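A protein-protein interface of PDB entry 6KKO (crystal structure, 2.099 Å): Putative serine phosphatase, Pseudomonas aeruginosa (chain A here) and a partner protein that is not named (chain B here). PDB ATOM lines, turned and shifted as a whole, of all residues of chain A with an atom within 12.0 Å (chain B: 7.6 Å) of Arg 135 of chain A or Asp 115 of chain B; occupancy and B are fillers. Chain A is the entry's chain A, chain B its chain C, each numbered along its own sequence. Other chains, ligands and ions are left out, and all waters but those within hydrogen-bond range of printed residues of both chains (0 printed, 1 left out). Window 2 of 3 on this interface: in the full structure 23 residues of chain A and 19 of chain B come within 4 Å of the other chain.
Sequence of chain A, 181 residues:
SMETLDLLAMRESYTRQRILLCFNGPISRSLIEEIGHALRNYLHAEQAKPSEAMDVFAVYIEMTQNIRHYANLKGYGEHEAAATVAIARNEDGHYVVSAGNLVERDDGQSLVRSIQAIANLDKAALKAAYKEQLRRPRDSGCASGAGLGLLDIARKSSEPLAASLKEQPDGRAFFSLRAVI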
ATOM      1  N   LEU A 126       4.592  -3.671 -12.438  1.00  0.00           N
ATOM      2  CA  LEU A 126       5.953  -3.273 -12.092  1.00  0.00           C
ATOM      3  C   LEU A 126       6.401  -3.916 -10.784  1.00  0.00           C
ATOM      4  O   LEU A 126       7.546  -4.363 -10.665  1.00  0.00           O
ATOM      5  CB  LEU A 126       6.050  -1.748 -12.005  1.00  0.00           C
ATOM      6  CG  LEU A 126       5.999  -0.953 -13.313  1.00  0.00           C
ATOM      7  CD1 LEU A 126       5.873   0.542 -13.035  1.00  0.00           C
ATOM      8  CD2 LEU A 126       7.217  -1.248 -14.182  1.00  0.00           C
ATOM      9  N   LYS A 127       5.508  -3.980  -9.793  1.00  0.00           N
ATOM     10  CA  LYS A 127       5.865  -4.605  -8.521  1.00  0.00           C
ATOM     11  C   LYS A 127       6.183  -6.083  -8.709  1.00  0.00           C
ATOM     12  O   LYS A 127       7.183  -6.587  -8.183  1.00  0.00           O
ATOM     13  CB  LYS A 127       4.735  -4.421  -7.505  1.00  0.00           C
ATOM     14  CG  LYS A 127       5.009  -5.045  -6.136  1.00  0.00           C
ATOM     15  CD  LYS A 127       3.942  -4.646  -5.120  1.00  0.00           C
ATOM     16  CE  LYS A 127       4.261  -5.165  -3.723  1.00  0.00           C
ATOM     17  NZ  LYS A 127       4.475  -6.641  -3.681  1.00  0.00           N
ATOM     18  N   ALA A 128       5.344  -6.792  -9.465  1.00  0.00           N
ATOM     19  CA  ALA A 128       5.569  -8.216  -9.685  1.00  0.00           C
ATOM     20  C   ALA A 128       6.901  -8.457 -10.386  1.00  0.00           C
ATOM     21  O   ALA A 128       7.684  -9.320  -9.973  1.00  0.00           O
ATOM     22  CB  ALA A 128       4.411  -8.809 -10.488  1.00  0.00           C
ATOM     23  N   ALA A 129       7.180  -7.693 -11.448  1.00  0.00           N
ATOM     24  CA  ALA A 129       8.459  -7.834 -12.139  1.00  0.00           C
ATOM     25  C   ALA A 129       9.624  -7.455 -11.231  1.00  0.00           C
ATOM     26  O   ALA A 129      10.694  -8.071 -11.290  1.00  0.00           O
ATOM     27  CB  ALA A 129       8.469  -6.986 -13.411  1.00  0.00           C
ATOM     28  N   TYR A 130       9.437  -6.438 -10.389  1.00  0.00           N
ATOM     29  CA  TYR A 130      10.453  -6.096  -9.398  1.00  0.00           C
ATOM     30  C   TYR A 130      10.665  -7.245  -8.424  1.00  0.00           C
ATOM     31  O   TYR A 130      11.799  -7.684  -8.198  1.00  0.00           O
ATOM     32  CB  TYR A 130      10.045  -4.830  -8.647  1.00  0.00           C
ATOM     33  CG  TYR A 130      11.035  -4.372  -7.597  1.00  0.00           C
ATOM     34  CD1 TYR A 130      10.974  -4.859  -6.297  1.00  0.00           C
ATOM     35  CD2 TYR A 130      12.015  -3.434  -7.901  1.00  0.00           C
ATOM     36  CE1 TYR A 130      11.870  -4.438  -5.331  1.00  0.00           C
ATOM     37  CE2 TYR A 130      12.918  -3.003  -6.939  1.00  0.00           C
ATOM     38  CZ  TYR A 130      12.839  -3.508  -5.654  1.00  0.00           C
ATOM     39  OH  TYR A 130      13.729  -3.085  -4.689  1.00  0.00           O
ATOM     40  N   LYS A 131       9.577  -7.720  -7.810  1.00  0.00           N
ATOM     41  CA  LYS A 131       9.674  -8.806  -6.843  1.00  0.00           C
ATOM     42  C   LYS A 131      10.246 -10.068  -7.469  1.00  0.00           C
ATOM     43  O   LYS A 131      10.915 -10.851  -6.784  1.00  0.00           O
ATOM     44  CB  LYS A 131       8.295  -9.081  -6.242  1.00  0.00           C
ATOM     45  CG  LYS A 131       8.315  -9.806  -4.911  1.00  0.00           C
ATOM     46  CD  LYS A 131       6.922  -9.858  -4.306  1.00  0.00           C
ATOM     47  CE  LYS A 131       5.942 -10.553  -5.243  1.00  0.00           C
ATOM     48  NZ  LYS A 131       6.357 -11.950  -5.561  1.00  0.00           N
ATOM     49  N   GLU A 132      10.009 -10.282  -8.765  1.00  0.00           N
ATOM     50  CA  GLU A 132      10.576 -11.451  -9.427  1.00  0.00           C
ATOM     51  C   GLU A 132      12.058 -11.278  -9.713  1.00  0.00           C
ATOM     52  O   GLU A 132      12.809 -12.263  -9.677  1.00  0.00           O
ATOM     53  CB  GLU A 132       9.810 -11.754 -10.714  1.00  0.00           C
ATOM     54  CG  GLU A 132       9.412 -13.213 -10.816  1.00  0.00           C
ATOM     55  CD  GLU A 132       8.746 -13.718  -9.548  1.00  0.00           C
ATOM     56  OE1 GLU A 132       9.118 -14.814  -9.076  1.00  0.00           O
ATOM     57  OE2 GLU A 132       7.871 -13.007  -9.007  1.00  0.00           O
ATOM     58  N   GLN A 133      12.504 -10.050  -9.993  1.00  0.00           N
ATOM     59  CA  GLN A 133      13.928  -9.832 -10.221  1.00  0.00           C
ATOM     60  C   GLN A 133      14.706  -9.792  -8.912  1.00  0.00           C
ATOM     61  O   GLN A 133      15.935  -9.877  -8.940  1.00  0.00           O
ATOM     62  CB  GLN A 133      14.140  -8.533 -11.018  1.00  0.00           C
ATOM     63  CG  GLN A 133      14.775  -8.718 -12.418  1.00  0.00           C
ATOM     64  CD  GLN A 133      16.269  -8.973 -12.396  1.00  0.00           C
ATOM     65  OE1 GLN A 133      16.841  -9.373 -11.381  1.00  0.00           O
ATOM     66  NE2 GLN A 133      16.914  -8.741 -13.526  1.00  0.00           N
ATOM     67  N   LEU A 134      14.014  -9.710  -7.771  1.00  0.00           N
ATOM     68  CA  LEU A 134      14.636  -9.923  -6.469  1.00  0.00           C
ATOM     69  C   LEU A 134      15.102 -11.350  -6.251  1.00  0.00           C
ATOM     70  O   LEU A 134      15.983 -11.575  -5.410  1.00  0.00           O
ATOM     71  CB  LEU A 134      13.692  -9.512  -5.331  1.00  0.00           C
ATOM     72  CG  LEU A 134      13.637  -8.013  -5.035  1.00  0.00           C
ATOM     73  CD1 LEU A 134      12.550  -7.674  -4.030  1.00  0.00           C
ATOM     74  CD2 LEU A 134      14.988  -7.563  -4.504  1.00  0.00           C
ATOM     75  N   ARG A 135      14.519 -12.313  -6.953  1.00  0.00           N
ATOM     76  CA  ARG A 135      14.855 -13.724  -6.750  1.00  0.00           C
ATOM     77  C   ARG A 135      15.655 -14.308  -7.898  1.00  0.00           C
ATOM     78  O   ARG A 135      16.088 -13.590  -8.785  1.00  0.00           O
ATOM     79  CB  ARG A 135      13.589 -14.551  -6.546  1.00  0.00           C
ATOM     80  CG  ARG A 135      12.709 -13.994  -5.446  1.00  0.00           C
ATOM     81  CD  ARG A 135      13.472 -14.066  -4.111  1.00  0.00           C
ATOM     82  NE  ARG A 135      12.691 -14.613  -3.009  1.00  0.00           N
ATOM     83  CZ  ARG A 135      13.145 -14.786  -1.769  1.00  0.00           C
ATOM     84  NH1 ARG A 135      14.374 -14.438  -1.403  1.00  0.00           N
ATOM     85  NH2 ARG A 135      12.330 -15.313  -0.863  1.00  0.00           N
ATOM     86  N   GLY A 145      17.230  -7.116 -20.688  1.00  0.00           N
ATOM     87  CA  GLY A 145      16.288  -7.374 -19.616  1.00  0.00           C
ATOM     88  C   GLY A 145      16.395  -6.377 -18.478  1.00  0.00           C
ATOM     89  O   GLY A 145      17.484  -6.105 -17.969  1.00  0.00           O
ATOM     90  N   ALA A 146      15.251  -5.834 -18.076  1.00  0.00           N
ATOM     91  CA  ALA A 146      15.218  -4.805 -17.048  1.00  0.00           C
ATOM     92  C   ALA A 146      15.370  -5.413 -15.660  1.00  0.00           C
ATOM     93  O   ALA A 146      14.732  -6.417 -15.327  1.00  0.00           O
ATOM     94  CB  ALA A 146      13.912  -4.026 -17.132  1.00  0.00           C
ATOM     95  N   GLY A 147      16.214  -4.786 -14.840  1.00  0.00           N
ATOM     96  CA  GLY A 147      16.465  -5.226 -13.491  1.00  0.00           C
ATOM     97  C   GLY A 147      15.917  -4.266 -12.452  1.00  0.00           C
ATOM     98  O   GLY A 147      15.128  -3.367 -12.747  1.00  0.00           O
ATOM     99  N   LEU A 148      16.377  -4.463 -11.210  1.00  0.00           N
ATOM    100  CA  LEU A 148      15.801  -3.745 -10.074  1.00  0.00           C
ATOM    101  C   LEU A 148      15.929  -2.236 -10.227  1.00  0.00           C
ATOM    102  O   LEU A 148      15.005  -1.494  -9.879  1.00  0.00           O
ATOM    103  CB  LEU A 148      16.469  -4.193  -8.773  1.00  0.00           C
ATOM    104  CG  LEU A 148      16.225  -5.609  -8.245  1.00  0.00           C
ATOM    105  CD1 LEU A 148      16.910  -5.757  -6.896  1.00  0.00           C
ATOM    106  CD2 LEU A 148      14.740  -5.934  -8.142  1.00  0.00           C
ATOM    107  N   GLY A 149      17.053  -1.760 -10.758  1.00  0.00           N
ATOM    108  CA  GLY A 149      17.273  -0.331 -10.876  1.00  0.00           C
ATOM    109  C   GLY A 149      16.257   0.365 -11.758  1.00  0.00           C
ATOM    110  O   GLY A 149      15.544   1.267 -11.299  1.00  0.00           O
ATOM    111  N   LEU A 151      13.551  -0.908 -12.850  1.00  0.00           N
ATOM    112  CA  LEU A 151      12.225  -1.212 -12.322  1.00  0.00           C
ATOM    113  C   LEU A 151      11.898  -0.334 -11.120  1.00  0.00           C
ATOM    114  O   LEU A 151      10.744   0.063 -10.937  1.00  0.00           O
ATOM    115  CB  LEU A 151      12.121  -2.691 -11.946  1.00  0.00           C
ATOM    116  CG  LEU A 151      11.989  -3.711 -13.082  1.00  0.00           C
ATOM    117  CD1 LEU A 151      12.028  -5.129 -12.527  1.00  0.00           C
ATOM    118  CD2 LEU A 151      10.714  -3.491 -13.899  1.00  0.00           C
ATOM    119  N   ARG A 155       8.914   2.391 -10.982  1.00  0.00           N
ATOM    120  CA  ARG A 155       7.907   2.338  -9.924  1.00  0.00           C
ATOM    121  C   ARG A 155       7.768   3.674  -9.204  1.00  0.00           C
ATOM    122  O   ARG A 155       6.671   4.024  -8.760  1.00  0.00           O
ATOM    123  CB  ARG A 155       8.241   1.229  -8.927  1.00  0.00           C
ATOM    124  CG  ARG A 155       7.977  -0.177  -9.459  1.00  0.00           C
ATOM    125  CD  ARG A 155       8.375  -1.223  -8.439  1.00  0.00           C
ATOM    126  NE  ARG A 155       7.549  -1.162  -7.238  1.00  0.00           N
ATOM    127  CZ  ARG A 155       7.798  -1.854  -6.131  1.00  0.00           C
ATOM    128  NH1 ARG A 155       8.861  -2.649  -6.069  1.00  0.00           N
ATOM    129  NH2 ARG A 155       6.993  -1.744  -5.083  1.00  0.00           N
ATOM    130  N   MET B  76      18.228  -8.951   1.347  1.00  0.00           N
ATOM    131  CA  MET B  76      17.503 -10.177   1.015  1.00  0.00           C
ATOM    132  C   MET B  76      18.310 -11.438   1.337  1.00  0.00           C
ATOM    133  O   MET B  76      17.752 -12.426   1.809  1.00  0.00           O
ATOM    134  CB  MET B  76      17.107 -10.183  -0.463  1.00  0.00           C
ATOM    135  CG  MET B  76      15.814  -9.436  -0.763  1.00  0.00           C
ATOM    136  SD  MET B  76      14.232 -10.303  -0.004  1.00  0.00           S
ATOM    137  CE  MET B  76      12.861  -9.071  -0.645  1.00  0.00           C
ATOM    138  N   ASP B  77      19.621 -11.402   1.077  1.00  0.00           N
ATOM    139  CA  ASP B  77      20.478 -12.526   1.450  1.00  0.00           C
ATOM    140  C   ASP B  77      20.486 -12.745   2.956  1.00  0.00           C
ATOM    141  O   ASP B  77      20.518 -13.890   3.422  1.00  0.00           O
ATOM    142  CB  ASP B  77      21.906 -12.310   0.948  1.00  0.00           C
ATOM    143  CG  ASP B  77      22.020 -12.442  -0.552  1.00  0.00           C
ATOM    144  OD1 ASP B  77      21.134 -13.079  -1.160  1.00  0.00           O
ATOM    145  OD2 ASP B  77      22.995 -11.915  -1.123  1.00  0.00           O
ATOM    146  N   LEU B  79      18.004 -11.907   5.068  1.00  0.00           N
ATOM    147  CA  LEU B  79      16.692 -12.405   5.467  1.00  0.00           C
ATOM    148  C   LEU B  79      16.461 -13.831   4.986  1.00  0.00           C
ATOM    149  O   LEU B  79      15.685 -14.569   5.604  1.00  0.00           O
ATOM    150  CB  LEU B  79      15.591 -11.476   4.959  1.00  0.00           C
ATOM    151  CG  LEU B  79      15.635 -10.029   5.470  1.00  0.00           C
ATOM    152  CD1 LEU B  79      14.276  -9.366   5.294  1.00  0.00           C
ATOM    153  CD2 LEU B  79      16.131  -9.925   6.912  1.00  0.00           C
ATOM    154  N   ASP B  80      17.117 -14.247   3.898  1.00  0.00           N
ATOM    155  CA  ASP B  80      17.025 -15.649   3.499  1.00  0.00           C
ATOM    156  C   ASP B  80      17.696 -16.564   4.515  1.00  0.00           C
ATOM    157  O   ASP B  80      17.246 -17.697   4.713  1.00  0.00           O
ATOM    158  CB  ASP B  80      17.652 -15.870   2.123  1.00  0.00           C
ATOM    159  CG  ASP B  80      16.796 -15.341   0.992  1.00  0.00           C
ATOM    160  OD1 ASP B  80      15.576 -15.166   1.195  1.00  0.00           O
ATOM    161  OD2 ASP B  80      17.347 -15.111  -0.106  1.00  0.00           O
ATOM    162  N   GLU B  83      15.169 -16.780   7.469  1.00  0.00           N
ATOM    163  CA  GLU B  83      14.027 -17.620   7.136  1.00  0.00           C
ATOM    164  C   GLU B  83      14.405 -19.094   7.147  1.00  0.00           C
ATOM    165  O   GLU B  83      13.637 -19.937   7.626  1.00  0.00           O
ATOM    166  CB  GLU B  83      13.479 -17.215   5.768  1.00  0.00           C
ATOM    167  CG  GLU B  83      12.318 -18.042   5.260  1.00  0.00           C
ATOM    168  CD  GLU B  83      11.047 -17.812   6.046  1.00  0.00           C
ATOM    169  OE1 GLU B  83      10.997 -16.859   6.849  1.00  0.00           O
ATOM    170  OE2 GLU B  83      10.087 -18.581   5.846  1.00  0.00           O
ATOM    171  N   LEU B 108       9.139  -0.324   2.038  1.00  0.00           N
ATOM    172  CA  LEU B 108      10.270  -1.199   1.740  1.00  0.00           C
ATOM    173  C   LEU B 108      10.354  -2.346   2.740  1.00  0.00           C
ATOM    174  O   LEU B 108      10.516  -3.511   2.354  1.00  0.00           O
ATOM    175  CB  LEU B 108      11.574  -0.396   1.750  1.00  0.00           C
ATOM    176  CG  LEU B 108      12.830  -1.259   1.608  1.00  0.00           C
ATOM    177  CD1 LEU B 108      12.839  -1.979   0.266  1.00  0.00           C
ATOM    178  CD2 LEU B 108      14.085  -0.428   1.784  1.00  0.00           C
ATOM    179  N   ALA B 109      10.235  -2.026   4.032  1.00  0.00           N
ATOM    180  CA  ALA B 109      10.240  -3.043   5.077  1.00  0.00           C
ATOM    181  C   ALA B 109       9.115  -4.046   4.882  1.00  0.00           C
ATOM    182  O   ALA B 109       9.278  -5.233   5.190  1.00  0.00           O
ATOM    183  CB  ALA B 109      10.100  -2.376   6.446  1.00  0.00           C
ATOM    184  N   GLU B 110       7.966  -3.584   4.379  1.00  0.00           N
ATOM    185  CA  GLU B 110       6.844  -4.485   4.148  1.00  0.00           C
ATOM    186  C   GLU B 110       7.125  -5.428   2.988  1.00  0.00           C
ATOM    187  O   GLU B 110       6.737  -6.598   3.030  1.00  0.00           O
ATOM    188  CB  GLU B 110       5.567  -3.687   3.891  1.00  0.00           C
ATOM    189  CG  GLU B 110       4.381  -4.549   3.447  1.00  0.00           C
ATOM    190  CD  GLU B 110       4.146  -5.762   4.349  1.00  0.00           C
ATOM    191  OE1 GLU B 110       4.193  -5.610   5.590  1.00  0.00           O
ATOM    192  OE2 GLU B 110       3.918  -6.870   3.817  1.00  0.00           O
ATOM    193  N   GLU B 111       7.804  -4.944   1.942  1.00  0.00           N
ATOM    194  CA  GLU B 111       8.121  -5.827   0.826  1.00  0.00           C
ATOM    195  C   GLU B 111       9.079  -6.931   1.257  1.00  0.00           C
ATOM    196  O   GLU B 111       8.916  -8.092   0.861  1.00  0.00           O
ATOM    197  CB  GLU B 111       8.692  -5.027  -0.346  1.00  0.00           C
ATOM    198  CG  GLU B 111       7.609  -4.294  -1.137  1.00  0.00           C
ATOM    199  CD  GLU B 111       8.090  -3.780  -2.481  1.00  0.00           C
ATOM    200  OE1 GLU B 111       8.815  -4.522  -3.175  1.00  0.00           O
ATOM    201  OE2 GLU B 111       7.720  -2.647  -2.857  1.00  0.00           O
ATOM    202  N   PHE B 112      10.056  -6.599   2.107  1.00  0.00           N
ATOM    203  CA  PHE B 112      10.904  -7.635   2.689  1.00  0.00           C
ATOM    204  C   PHE B 112      10.079  -8.620   3.508  1.00  0.00           C
ATOM    205  O   PHE B 112      10.321  -9.832   3.466  1.00  0.00           O
ATOM    206  CB  PHE B 112      11.986  -7.009   3.568  1.00  0.00           C
ATOM    207  CG  PHE B 112      13.155  -6.439   2.804  1.00  0.00           C
ATOM    208  CD1 PHE B 112      14.086  -7.274   2.209  1.00  0.00           C
ATOM    209  CD2 PHE B 112      13.335  -5.066   2.711  1.00  0.00           C
ATOM    210  CE1 PHE B 112      15.172  -6.749   1.515  1.00  0.00           C
ATOM    211  CE2 PHE B 112      14.420  -4.538   2.021  1.00  0.00           C
ATOM    212  CZ  PHE B 112      15.335  -5.381   1.424  1.00  0.00           C
ATOM    213  N   ARG B 113       9.081  -8.125   4.242  1.00  0.00           N
ATOM    214  CA  ARG B 113       8.387  -8.988   5.185  1.00  0.00           C
ATOM    215  C   ARG B 113       7.441  -9.953   4.479  1.00  0.00           C
ATOM    216  O   ARG B 113       7.099 -10.996   5.050  1.00  0.00           O
ATOM    217  CB  ARG B 113       7.635  -8.128   6.211  1.00  0.00           C
ATOM    218  CG  ARG B 113       6.753  -8.900   7.196  1.00  0.00           C
ATOM    219  CD  ARG B 113       6.232  -8.000   8.307  1.00  0.00           C
ATOM    220  NE  ARG B 113       5.303  -6.990   7.810  1.00  0.00           N
ATOM    221  CZ  ARG B 113       4.691  -6.097   8.584  1.00  0.00           C
ATOM    222  NH1 ARG B 113       4.909  -6.088   9.892  1.00  0.00           N
ATOM    223  NH2 ARG B 113       3.855  -5.219   8.049  1.00  0.00           N
ATOM    224  N   GLU B 114       7.063  -9.671   3.229  1.00  0.00           N
ATOM    225  CA  GLU B 114       6.209 -10.609   2.511  1.00  0.00           C
ATOM    226  C   GLU B 114       6.949 -11.877   2.109  1.00  0.00           C
ATOM    227  O   GLU B 114       6.300 -12.880   1.809  1.00  0.00           O
ATOM    228  CB  GLU B 114       5.611  -9.957   1.263  1.00  0.00           C
ATOM    229  CG  GLU B 114       4.962  -8.610   1.484  1.00  0.00           C
ATOM    230  CD  GLU B 114       4.626  -7.907   0.180  1.00  0.00           C
ATOM    231  OE1 GLU B 114       5.287  -8.186  -0.845  1.00  0.00           O
ATOM    232  OE2 GLU B 114       3.690  -7.081   0.178  1.00  0.00           O
ATOM    233  N   ASP B 115       8.283 -11.861   2.101  1.00  0.00           N
ATOM    234  CA  ASP B 115       9.075 -13.048   1.814  1.00  0.00           C
ATOM    235  C   ASP B 115       9.600 -13.710   3.082  1.00  0.00           C
ATOM    236  O   ASP B 115      10.530 -14.522   3.014  1.00  0.00           O
ATOM    237  CB  ASP B 115      10.239 -12.708   0.881  1.00  0.00           C
ATOM    238  CG  ASP B 115       9.839 -11.763  -0.233  1.00  0.00           C
ATOM    239  OD1 ASP B 115       9.252 -12.229  -1.233  1.00  0.00           O
ATOM    240  OD2 ASP B 115      10.125 -10.553  -0.110  1.00  0.00           O
ATOM    241  N   CYS B 116       9.033 -13.367   4.233  1.00  0.00           N
ATOM    242  CA  CYS B 116       9.463 -13.884   5.521  1.00  0.00           C
ATOM    243  C   CYS B 116       8.259 -14.442   6.252  1.00  0.00           C
ATOM    244  O   CYS B 116       7.157 -13.890   6.163  1.00  0.00           O
ATOM    245  CB  CYS B 116      10.103 -12.796   6.384  1.00  0.00           C
ATOM    246  SG  CYS B 116      11.382 -11.889   5.553  1.00  0.00           S
ATOM    247  N   SER B 117       8.473 -15.521   6.995  1.00  0.00           N
ATOM    248  CA  SER B 117       7.412 -16.099   7.809  1.00  0.00           C
ATOM    249  C   SER B 117       7.745 -16.075   9.295  1.00  0.00           C
ATOM    250  O   SER B 117       7.019 -16.688  10.087  1.00  0.00           O
ATOM    251  CB  SER B 117       7.107 -17.528   7.346  1.00  0.00           C
ATOM    252  OG  SER B 117       8.283 -18.311   7.304  1.00  0.00           O
ATOM    253  N   PHE B 118       8.824 -15.380   9.693  1.00  0.00           N
ATOM    254  CA  PHE B 118       9.232 -15.214  11.081  1.00  0.00           C
ATOM    255  C   PHE B 118       8.705 -13.897  11.635  1.00  0.00           C
ATOM    256  O   PHE B 118       8.280 -13.024  10.873  1.00  0.00           O
ATOM    257  CB  PHE B 118      10.765 -15.266  11.197  1.00  0.00           C
ATOM    258  CG  PHE B 118      11.485 -14.311  10.284  1.00  0.00           C
ATOM    259  CD1 PHE B 118      11.586 -12.961  10.602  1.00  0.00           C
ATOM    260  CD2 PHE B 118      12.092 -14.766   9.124  1.00  0.00           C
ATOM    261  CE1 PHE B 118      12.253 -12.087   9.772  1.00  0.00           C
ATOM    262  CE2 PHE B 118      12.770 -13.893   8.288  1.00  0.00           C
ATOM    263  CZ  PHE B 118      12.848 -12.553   8.612  1.00  0.00           C
ATOM    264  N   PHE B 120       8.180 -10.328  12.415  1.00  0.00           N
ATOM    265  CA  PHE B 120       8.730  -9.199  11.669  1.00  0.00           C
ATOM    266  C   PHE B 120       7.847  -7.998  11.986  1.00  0.00           C
ATOM    267  O   PHE B 120       6.701  -7.933  11.531  1.00  0.00           O
ATOM    268  CB  PHE B 120       8.753  -9.511  10.166  1.00  0.00           C
ATOM    269  CG  PHE B 120       9.558  -8.537   9.317  1.00  0.00           C
ATOM    270  CD1 PHE B 120       9.439  -7.160   9.478  1.00  0.00           C
ATOM    271  CD2 PHE B 120      10.392  -9.014   8.313  1.00  0.00           C
ATOM    272  CE1 PHE B 120      10.162  -6.282   8.687  1.00  0.00           C
ATOM    273  CE2 PHE B 120      11.123  -8.133   7.511  1.00  0.00           C
ATOM    274  CZ  PHE B 120      11.002  -6.767   7.701  1.00  0.00           C
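The guanidinium group of Arg 155 of chain A is in salt-bridge range of the side-chain carboxylate of Glu 111 of chain B.
The guanidinium group of Arg 135 of chain A is in salt-bridge range of the side-chain carboxylate of Asp 80 of chain B, 3.0 Å away.
The side-chain amino group (NZ) of Lys 127 of chain A is in salt-bridge range of the side-chain carboxylate (OE1) of Glu 114 of chain B, 3.3 Å away.
Among the printed residues, pairs that only touch across the chains: Leu 134 of chain A with Met 76 of chain B, Tyr 130 of chain A with Glu 111 of chain B and Arg 135 of chain A with Asp 115 of chain B.
Of chain B, only Asp 80 (3.0 Å) and Asp 115 (3.8 Å) come within 4 Å of Arg 135 of chain A.
Asp 115 of chain B touches just one residue of chain A: Arg 135.
Printed residues of chain A within 4 Å of Asp 80 of chain B: Arg 135 (3.0 Å).
No residue of chain A comes within 4 Å of Glu 83 of chain B.
No residue of chain A comes within 4 Å of Phe 112 of chain B.
Glu 114 of chain B touches just one residue of chain A: Lys 127 (3.3 Å).
No residue of chain A comes within 4 Å of Cys 116 of chain B.
Printed residues of chain B within 4 Å of Leu 134 of chain A: Met 76 (3.7 Å).
Of the printed residues of chain A, Glu 111 of chain B touches Tyr 130 and Arg 155.
Of the printed residues of chain B, Arg 155 of chain A touches Glu 111 (2.5 Å).
Of the printed residues of chain B, Tyr 130 of chain A touches Glu 111.
Ala 129 of chain A touches none of the printed residues of chain B.
The nearest residue of chain B that does not touch Arg 135 of chain A is Met 76 of chain B (4.4 Å).
The nearest residue of chain A that does not touch Asp 115 of chain B is Lys 131 of chain A (4.5 Å).
The nearest printed residue of chain B that does not touch Tyr 130 of chain A is Leu 108 of chain B (5.2 Å).
Of the 17 printed residues of chain B, 5 touch a printed residue of chain A.
Hydrophobic or aromatic side chains of chain B that line the printed part of chain A: Met 76.
Hydrophobic or aromatic side chains of chain A that line the printed part of chain B: Tyr 130 and Leu 134.
Among the printed residues, 6 pairs touch across the chains.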
